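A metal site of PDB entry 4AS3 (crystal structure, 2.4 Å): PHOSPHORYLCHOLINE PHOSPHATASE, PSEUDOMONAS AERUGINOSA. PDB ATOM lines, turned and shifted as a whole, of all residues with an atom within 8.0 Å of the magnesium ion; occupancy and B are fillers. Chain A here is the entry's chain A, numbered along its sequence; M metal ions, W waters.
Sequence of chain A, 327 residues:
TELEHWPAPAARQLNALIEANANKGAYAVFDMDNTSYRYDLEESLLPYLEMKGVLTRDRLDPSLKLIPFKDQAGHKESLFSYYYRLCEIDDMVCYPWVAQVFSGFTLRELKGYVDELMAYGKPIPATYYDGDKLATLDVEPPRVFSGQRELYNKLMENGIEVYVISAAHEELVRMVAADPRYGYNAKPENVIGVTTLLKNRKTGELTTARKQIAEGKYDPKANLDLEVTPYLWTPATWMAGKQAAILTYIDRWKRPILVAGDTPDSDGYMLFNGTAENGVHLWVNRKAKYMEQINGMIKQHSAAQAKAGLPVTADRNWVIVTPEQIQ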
ATOM      1  N   PHE A  30      27.392  -6.797 -13.948  1.00  0.00           N
ATOM      2  CA  PHE A  30      28.046  -5.702 -14.689  1.00  0.00           C
ATOM      3  C   PHE A  30      27.759  -5.816 -16.162  1.00  0.00           C
ATOM      4  O   PHE A  30      27.941  -6.885 -16.713  1.00  0.00           O
ATOM      5  CB  PHE A  30      29.564  -5.805 -14.575  1.00  0.00           C
ATOM      6  CG  PHE A  30      30.102  -5.314 -13.284  1.00  0.00           C
ATOM      7  CD1 PHE A  30      30.089  -6.130 -12.160  1.00  0.00           C
ATOM      8  CD2 PHE A  30      30.656  -4.040 -13.190  1.00  0.00           C
ATOM      9  CE1 PHE A  30      30.595  -5.661 -10.946  1.00  0.00           C
ATOM     10  CE2 PHE A  30      31.142  -3.574 -11.983  1.00  0.00           C
ATOM     11  CZ  PHE A  30      31.122  -4.383 -10.857  1.00  0.00           C
ATOM     12  N   ASP A  31      27.366  -4.737 -16.820  1.00  0.00           N
ATOM     13  CA  ASP A  31      27.408  -4.760 -18.279  1.00  0.00           C
ATOM     14  C   ASP A  31      28.898  -4.725 -18.619  1.00  0.00           C
ATOM     15  O   ASP A  31      29.704  -4.364 -17.774  1.00  0.00           O
ATOM     16  CB  ASP A  31      26.640  -3.577 -18.910  1.00  0.00           C
ATOM     17  CG  ASP A  31      26.922  -3.425 -20.404  1.00  0.00           C
ATOM     18  OD1 ASP A  31      26.618  -4.369 -21.175  1.00  0.00           O
ATOM     19  OD2 ASP A  31      27.428  -2.359 -20.829  1.00  0.00           O
ATOM     20  N   MET A  32      29.277  -5.148 -19.805  1.00  0.00           N
ATOM     21  CA  MET A  32      30.702  -5.074 -20.199  1.00  0.00           C
ATOM     22  C   MET A  32      31.076  -3.836 -21.042  1.00  0.00           C
ATOM     23  O   MET A  32      31.854  -2.972 -20.616  1.00  0.00           O
ATOM     24  CB  MET A  32      31.122  -6.318 -20.985  1.00  0.00           C
ATOM     25  CG  MET A  32      32.614  -6.571 -20.964  1.00  0.00           C
ATOM     26  SD  MET A  32      33.043  -7.310 -19.391  1.00  0.00           S
ATOM     27  CE  MET A  32      34.763  -6.890 -19.089  1.00  0.00           C
ATOM     28  N   ASP A  33      30.570  -3.775 -22.264  1.00  0.00           N
ATOM     29  CA  ASP A  33      30.997  -2.674 -23.139  1.00  0.00           C
ATOM     30  C   ASP A  33      30.628  -1.288 -22.603  1.00  0.00           C
ATOM     31  O   ASP A  33      29.452  -1.017 -22.281  1.00  0.00           O
ATOM     32  CB  ASP A  33      30.482  -2.845 -24.561  1.00  0.00           C
ATOM     33  CG  ASP A  33      31.020  -4.088 -25.202  1.00  0.00           C
ATOM     34  OD1 ASP A  33      32.241  -4.150 -25.533  1.00  0.00           O
ATOM     35  OD2 ASP A  33      30.216  -5.028 -25.385  1.00  0.00           O
ATOM     36  N   ASN A  34      31.637  -0.432 -22.490  1.00  0.00           N
ATOM     37  CA  ASN A  34      31.403   0.954 -22.056  1.00  0.00           C
ATOM     38  C   ASN A  34      30.975   1.022 -20.592  1.00  0.00           C
ATOM     39  O   ASN A  34      30.576   2.050 -20.117  1.00  0.00           O
ATOM     40  CB  ASN A  34      30.382   1.638 -22.980  1.00  0.00           C
ATOM     41  CG  ASN A  34      31.032   2.250 -24.206  1.00  0.00           C
ATOM     42  OD1 ASN A  34      31.938   3.094 -24.091  1.00  0.00           O
ATOM     43  ND2 ASN A  34      30.566   1.863 -25.381  1.00  0.00           N
ATOM     44  N   THR A  35      31.080  -0.095 -19.900  1.00  0.00           N
ATOM     45  CA  THR A  35      30.832  -0.151 -18.441  1.00  0.00           C
ATOM     46  C   THR A  35      32.037  -0.741 -17.699  1.00  0.00           C
ATOM     47  O   THR A  35      32.540  -0.217 -16.699  1.00  0.00           O
ATOM     48  CB  THR A  35      29.560  -1.000 -18.146  1.00  0.00           C
ATOM     49  OG1 THR A  35      28.411  -0.400 -18.789  1.00  0.00           O
ATOM     50  CG2 THR A  35      29.309  -1.106 -16.667  1.00  0.00           C
ATOM     51  N   SER A  36      32.472  -1.875 -18.172  1.00  0.00           N
ATOM     52  CA  SER A  36      33.593  -2.516 -17.523  1.00  0.00           C
ATOM     53  C   SER A  36      34.904  -2.049 -18.116  1.00  0.00           C
ATOM     54  O   SER A  36      35.902  -1.949 -17.399  1.00  0.00           O
ATOM     55  CB  SER A  36      33.428  -4.017 -17.610  1.00  0.00           C
ATOM     56  OG  SER A  36      32.487  -4.394 -16.603  1.00  0.00           O
ATOM     57  N   TYR A  37      34.887  -1.753 -19.417  1.00  0.00           N
ATOM     58  CA  TYR A  37      35.971  -1.043 -20.094  1.00  0.00           C
ATOM     59  C   TYR A  37      35.356   0.018 -20.932  1.00  0.00           C
ATOM     60  O   TYR A  37      34.152  -0.032 -21.204  1.00  0.00           O
ATOM     61  CB  TYR A  37      36.791  -1.946 -21.031  1.00  0.00           C
ATOM     62  CG  TYR A  37      36.003  -2.895 -21.893  1.00  0.00           C
ATOM     63  CD1 TYR A  37      35.275  -2.468 -23.021  1.00  0.00           C
ATOM     64  CD2 TYR A  37      36.014  -4.251 -21.609  1.00  0.00           C
ATOM     65  CE1 TYR A  37      34.559  -3.372 -23.808  1.00  0.00           C
ATOM     66  CE2 TYR A  37      35.313  -5.152 -22.402  1.00  0.00           C
ATOM     67  CZ  TYR A  37      34.575  -4.714 -23.504  1.00  0.00           C
ATOM     68  OH  TYR A  37      33.886  -5.708 -24.272  1.00  0.00           O
ATOM     69  N   TYR A  39      34.650   1.980 -24.472  1.00  0.00           N
ATOM     70  CA  TYR A  39      34.347   1.637 -25.870  1.00  0.00           C
ATOM     71  C   TYR A  39      33.799   0.231 -25.972  1.00  0.00           C
ATOM     72  O   TYR A  39      33.556  -0.413 -24.934  1.00  0.00           O
ATOM     73  CB  TYR A  39      35.545   1.891 -26.828  1.00  0.00           C
ATOM     74  CG  TYR A  39      36.220   3.241 -26.551  1.00  0.00           C
ATOM     75  CD1 TYR A  39      35.545   4.447 -26.802  1.00  0.00           C
ATOM     76  CD2 TYR A  39      37.514   3.300 -26.010  1.00  0.00           C
ATOM     77  CE1 TYR A  39      36.127   5.667 -26.510  1.00  0.00           C
ATOM     78  CE2 TYR A  39      38.111   4.530 -25.709  1.00  0.00           C
ATOM     79  CZ  TYR A  39      37.416   5.705 -25.958  1.00  0.00           C
ATOM     80  OH  TYR A  39      37.995   6.895 -25.671  1.00  0.00           O
ATOM     81  N   ASP A  40      33.668  -0.264 -27.196  1.00  0.00           N
ATOM     82  CA  ASP A  40      32.878  -1.442 -27.473  1.00  0.00           C
ATOM     83  C   ASP A  40      33.725  -2.525 -28.219  1.00  0.00           C
ATOM     84  O   ASP A  40      34.445  -2.212 -29.176  1.00  0.00           O
ATOM     85  CB  ASP A  40      31.701  -0.974 -28.339  1.00  0.00           C
ATOM     86  CG  ASP A  40      30.644  -2.054 -28.508  1.00  0.00           C
ATOM     87  OD1 ASP A  40      29.730  -2.159 -27.644  1.00  0.00           O
ATOM     88  OD2 ASP A  40      30.675  -2.776 -29.519  1.00  0.00           O
ATOM     89  N   ILE A 165      26.757  -9.500 -17.631  1.00  0.00           N
ATOM     90  CA  ILE A 165      25.597  -9.699 -18.530  1.00  0.00           C
ATOM     91  C   ILE A 165      25.679  -8.614 -19.593  1.00  0.00           C
ATOM     92  O   ILE A 165      25.357  -7.472 -19.328  1.00  0.00           O
ATOM     93  CB  ILE A 165      24.208  -9.706 -17.806  1.00  0.00           C
ATOM     94  CG1 ILE A 165      24.217 -10.791 -16.686  1.00  0.00           C
ATOM     95  CG2 ILE A 165      23.105  -9.918 -18.823  1.00  0.00           C
ATOM     96  CD1 ILE A 165      22.895 -11.064 -15.975  1.00  0.00           C
ATOM     97  N   SER A 166      26.081  -9.043 -20.786  1.00  0.00           N
ATOM     98  CA  SER A 166      26.440  -8.266 -21.923  1.00  0.00           C
ATOM     99  C   SER A 166      25.559  -8.605 -23.097  1.00  0.00           C
ATOM    100  O   SER A 166      25.113  -9.750 -23.248  1.00  0.00           O
ATOM    101  CB  SER A 166      27.859  -8.656 -22.312  1.00  0.00           C
ATOM    102  OG  SER A 166      28.191  -8.079 -23.567  1.00  0.00           O
ATOM    103  N   ALA A 167      25.367  -7.595 -23.946  1.00  0.00           N
ATOM    104  CA  ALA A 167      24.659  -7.717 -25.231  1.00  0.00           C
ATOM    105  C   ALA A 167      25.594  -8.092 -26.401  1.00  0.00           C
ATOM    106  O   ALA A 167      25.121  -8.368 -27.498  1.00  0.00           O
ATOM    107  CB  ALA A 167      23.889  -6.452 -25.557  1.00  0.00           C
ATOM    108  N   ALA A 168      26.894  -8.113 -26.152  1.00  0.00           N
ATOM    109  CA  ALA A 168      27.901  -8.692 -27.038  1.00  0.00           C
ATOM    110  C   ALA A 168      27.919 -10.238 -26.895  1.00  0.00           C
ATOM    111  O   ALA A 168      27.394 -10.784 -25.903  1.00  0.00           O
ATOM    112  CB  ALA A 168      29.276  -8.121 -26.724  1.00  0.00           C
ATOM    113  N   LYS A 242      18.204  -9.152 -20.239  1.00  0.00           N
ATOM    114  CA  LYS A 242      19.221  -9.131 -19.214  1.00  0.00           C
ATOM    115  C   LYS A 242      18.610  -9.571 -17.879  1.00  0.00           C
ATOM    116  O   LYS A 242      19.244 -10.332 -17.115  1.00  0.00           O
ATOM    117  CB  LYS A 242      19.857  -7.736 -19.084  1.00  0.00           C
ATOM    118  CG  LYS A 242      20.707  -7.335 -20.286  1.00  0.00           C
ATOM    119  CD  LYS A 242      21.911  -6.452 -19.915  1.00  0.00           C
ATOM    120  CE  LYS A 242      22.634  -5.997 -21.179  1.00  0.00           C
ATOM    121  NZ  LYS A 242      23.888  -5.227 -20.887  1.00  0.00           N
ATOM    122  N   ALA A 260      25.503  -2.649 -12.862  1.00  0.00           N
ATOM    123  CA  ALA A 260      26.258  -1.612 -13.560  1.00  0.00           C
ATOM    124  C   ALA A 260      25.938  -1.570 -15.056  1.00  0.00           C
ATOM    125  O   ALA A 260      25.930  -2.621 -15.703  1.00  0.00           O
ATOM    126  CB  ALA A 260      27.739  -1.811 -13.320  1.00  0.00           C
ATOM    127  N   GLY A 261      25.758  -0.356 -15.591  1.00  0.00           N
ATOM    128  CA  GLY A 261      25.260  -0.089 -16.937  1.00  0.00           C
ATOM    129  C   GLY A 261      25.696   1.287 -17.465  1.00  0.00           C
ATOM    130  O   GLY A 261      26.293   2.071 -16.746  1.00  0.00           O
ATOM    131  N   ASP A 262      25.420   1.521 -18.749  1.00  0.00           N
ATOM    132  CA  ASP A 262      25.817   2.711 -19.437  1.00  0.00           C
ATOM    133  C   ASP A 262      24.856   2.996 -20.582  1.00  0.00           C
ATOM    134  O   ASP A 262      24.891   4.049 -21.178  1.00  0.00           O
ATOM    135  CB  ASP A 262      27.228   2.520 -20.027  1.00  0.00           C
ATOM    136  CG  ASP A 262      27.230   1.628 -21.279  1.00  0.00           C
ATOM    137  OD1 ASP A 262      27.282   0.389 -21.133  1.00  0.00           O
ATOM    138  OD2 ASP A 262      27.195   2.180 -22.411  1.00  0.00           O
ATOM    139  N   THR A 263      24.021   2.020 -20.940  1.00  0.00           N
ATOM    140  CA  THR A 263      23.062   2.236 -22.027  1.00  0.00           C
ATOM    141  C   THR A 263      21.588   2.213 -21.528  1.00  0.00           C
ATOM    142  O   THR A 263      21.090   1.119 -21.126  1.00  0.00           O
ATOM    143  CB  THR A 263      23.193   1.140 -23.109  1.00  0.00           C
ATOM    144  OG1 THR A 263      24.537   1.139 -23.551  1.00  0.00           O
ATOM    145  CG2 THR A 263      22.237   1.388 -24.306  1.00  0.00           C
ATOM    146  N   SER A 266      19.135  -0.663 -23.232  1.00  0.00           N
ATOM    147  CA  SER A 266      19.642  -2.002 -23.067  1.00  0.00           C
ATOM    148  C   SER A 266      19.886  -2.437 -21.605  1.00  0.00           C
ATOM    149  O   SER A 266      19.659  -3.587 -21.255  1.00  0.00           O
ATOM    150  CB  SER A 266      20.882  -2.227 -23.900  1.00  0.00           C
ATOM    151  OG  SER A 266      21.243  -3.595 -23.867  1.00  0.00           O
ATOM    152  N   ASP A 267      20.404  -1.549 -20.774  1.00  0.00           N
ATOM    153  CA  ASP A 267      20.680  -1.918 -19.398  1.00  0.00           C
ATOM    154  C   ASP A 267      19.484  -1.613 -18.398  1.00  0.00           C
ATOM    155  O   ASP A 267      19.525  -2.018 -17.226  1.00  0.00           O
ATOM    156  CB  ASP A 267      21.986  -1.241 -18.944  1.00  0.00           C
ATOM    157  CG  ASP A 267      23.225  -1.690 -19.775  1.00  0.00           C
ATOM    158  OD1 ASP A 267      23.375  -2.922 -20.037  1.00  0.00           O
ATOM    159  OD2 ASP A 267      24.090  -0.813 -20.125  1.00  0.00           O
ATOM    160  N   MET A 270      17.645  -4.555 -16.248  1.00  0.00           N
ATOM    161  CA  MET A 270      18.361  -5.103 -15.069  1.00  0.00           C
ATOM    162  C   MET A 270      18.616  -4.031 -14.016  1.00  0.00           C
ATOM    163  O   MET A 270      18.612  -4.316 -12.828  1.00  0.00           O
ATOM    164  CB  MET A 270      19.633  -5.896 -15.388  1.00  0.00           C
ATOM    165  CG  MET A 270      20.745  -5.065 -16.008  1.00  0.00           C
ATOM    166  SD  MET A 270      22.171  -6.099 -16.352  1.00  0.00           S
ATOM    167  CE  MET A 270      23.452  -4.876 -16.663  1.00  0.00           C
ATOM    168  N   VAL A 284      27.858   4.378 -15.600  1.00  0.00           N
ATOM    169  CA  VAL A 284      28.977   5.012 -16.283  1.00  0.00           C
ATOM    170  C   VAL A 284      28.393   5.955 -17.344  1.00  0.00           C
ATOM    171  O   VAL A 284      27.731   5.505 -18.290  1.00  0.00           O
ATOM    172  CB  VAL A 284      29.920   3.941 -16.952  1.00  0.00           C
ATOM    173  CG1 VAL A 284      31.067   4.599 -17.731  1.00  0.00           C
ATOM    174  CG2 VAL A 284      30.512   2.995 -15.902  1.00  0.00           C
ATOM    175  N   ARG A 286      28.767   8.106 -20.425  1.00  0.00           N
ATOM    176  CA  ARG A 286      29.684   8.287 -21.560  1.00  0.00           C
ATOM    177  C   ARG A 286      29.050   9.022 -22.739  1.00  0.00           C
ATOM    178  O   ARG A 286      29.556   8.930 -23.851  1.00  0.00           O
ATOM    179  CB  ARG A 286      30.194   6.925 -22.060  1.00  0.00           C
ATOM    180  CG  ARG A 286      29.122   5.875 -22.287  1.00  0.00           C
ATOM    181  CD  ARG A 286      28.902   5.528 -23.746  1.00  0.00           C
ATOM    182  NE  ARG A 286      27.997   4.394 -23.916  1.00  0.00           N
ATOM    183  CZ  ARG A 286      27.405   4.098 -25.088  1.00  0.00           C
ATOM    184  NH1 ARG A 286      27.637   4.860 -26.183  1.00  0.00           N
ATOM    185  NH2 ARG A 286      26.570   3.051 -25.184  1.00  0.00           N
ATOM    186  N   TYR A 290      22.503  10.225 -22.973  1.00  0.00           N
ATOM    187  CA  TYR A 290      22.170   9.068 -22.137  1.00  0.00           C
ATOM    188  C   TYR A 290      21.957   9.423 -20.645  1.00  0.00           C
ATOM    189  O   TYR A 290      21.140   8.785 -19.991  1.00  0.00           O
ATOM    190  CB  TYR A 290      23.167   7.909 -22.297  1.00  0.00           C
ATOM    191  CG  TYR A 290      23.080   7.130 -23.607  1.00  0.00           C
ATOM    192  CD1 TYR A 290      22.050   7.333 -24.524  1.00  0.00           C
ATOM    193  CD2 TYR A 290      24.000   6.111 -23.877  1.00  0.00           C
ATOM    194  CE1 TYR A 290      21.943   6.586 -25.708  1.00  0.00           C
ATOM    195  CE2 TYR A 290      23.932   5.361 -25.076  1.00  0.00           C
ATOM    196  CZ  TYR A 290      22.913   5.611 -25.977  1.00  0.00           C
ATOM    197  OH  TYR A 290      22.846   4.879 -27.133  1.00  0.00           O
HETATM  198 MG    MG M   1      27.495  -1.213 -22.473  1.00  0.00          MG
HETATM  199  O   HOH W   1      27.280  -3.288 -23.574  1.00  0.00           O
HETATM  200  O   HOH W   2      25.436  -1.329 -22.134  1.00  0.00           O
HETATM  201  O   HOH W   3      27.419   0.268 -23.847  1.00  0.00           O
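The side-chain carboxylate (OD2) of Asp 31 sits close to the side-chain hydroxyl (OG1) of Thr 35, 3.0 Å away.
The backbone NH of Asp 262 sits at hydrogen-bond distance from the side-chain carboxylate of Asp 267, 3.0 Å away.
The side-chain carboxylate (OD1) of Asp 31 lies within salt-bridge range of the side-chain amino group (NZ) of Lys 242.
The side-chain hydroxyl (OG) of Ser 36 sits at hydrogen-bond distance from the backbone carbonyl oxygen (O) of Asp 31.
OG1 of Thr 263 lies within hydrogen-bond range of NH2 of Arg 286, 3.2 Å away.
N of Thr 263 lies within hydrogen-bond range of OD2 of Asp 267 (2.9 Å).
OD1 of Asp 262 lies close to OG1 of Thr 35 (2.7 Å).
The backbone carbonyl oxygen (O) of Ala 260 lies within hydrogen-bond range of the backbone NH (N) of Asp 31, 2.8 Å away.
OG1 of Thr 35 touches the magnesium ion (3.9 Å).
OG1 of Thr 263 touches the magnesium ion (3.9 Å).
Five residues have an atom within 4 Å of the magnesium ion: Asp 31, Asp 33, Thr 35, Asp 262 and Thr 263.
The magnesium ion is bound by O of Asp 33, OD2 of Asp 31, water W3, water W2, OD1 of Asp 262 and water W1.
Water W3 lies within hydrogen-bond range of the side-chain carboxylate (OD2) of Asp 262, the side-chain hydroxyl (OG1) of Thr 263 and the guanidinium group (NH2) of Arg 286.
Water W2 lies within hydrogen-bond range of OD2 of Asp 267 (2.5 Å), OG1 of Thr 263 (3.0 Å) and OD1 of Asp 31 (3.4 Å).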
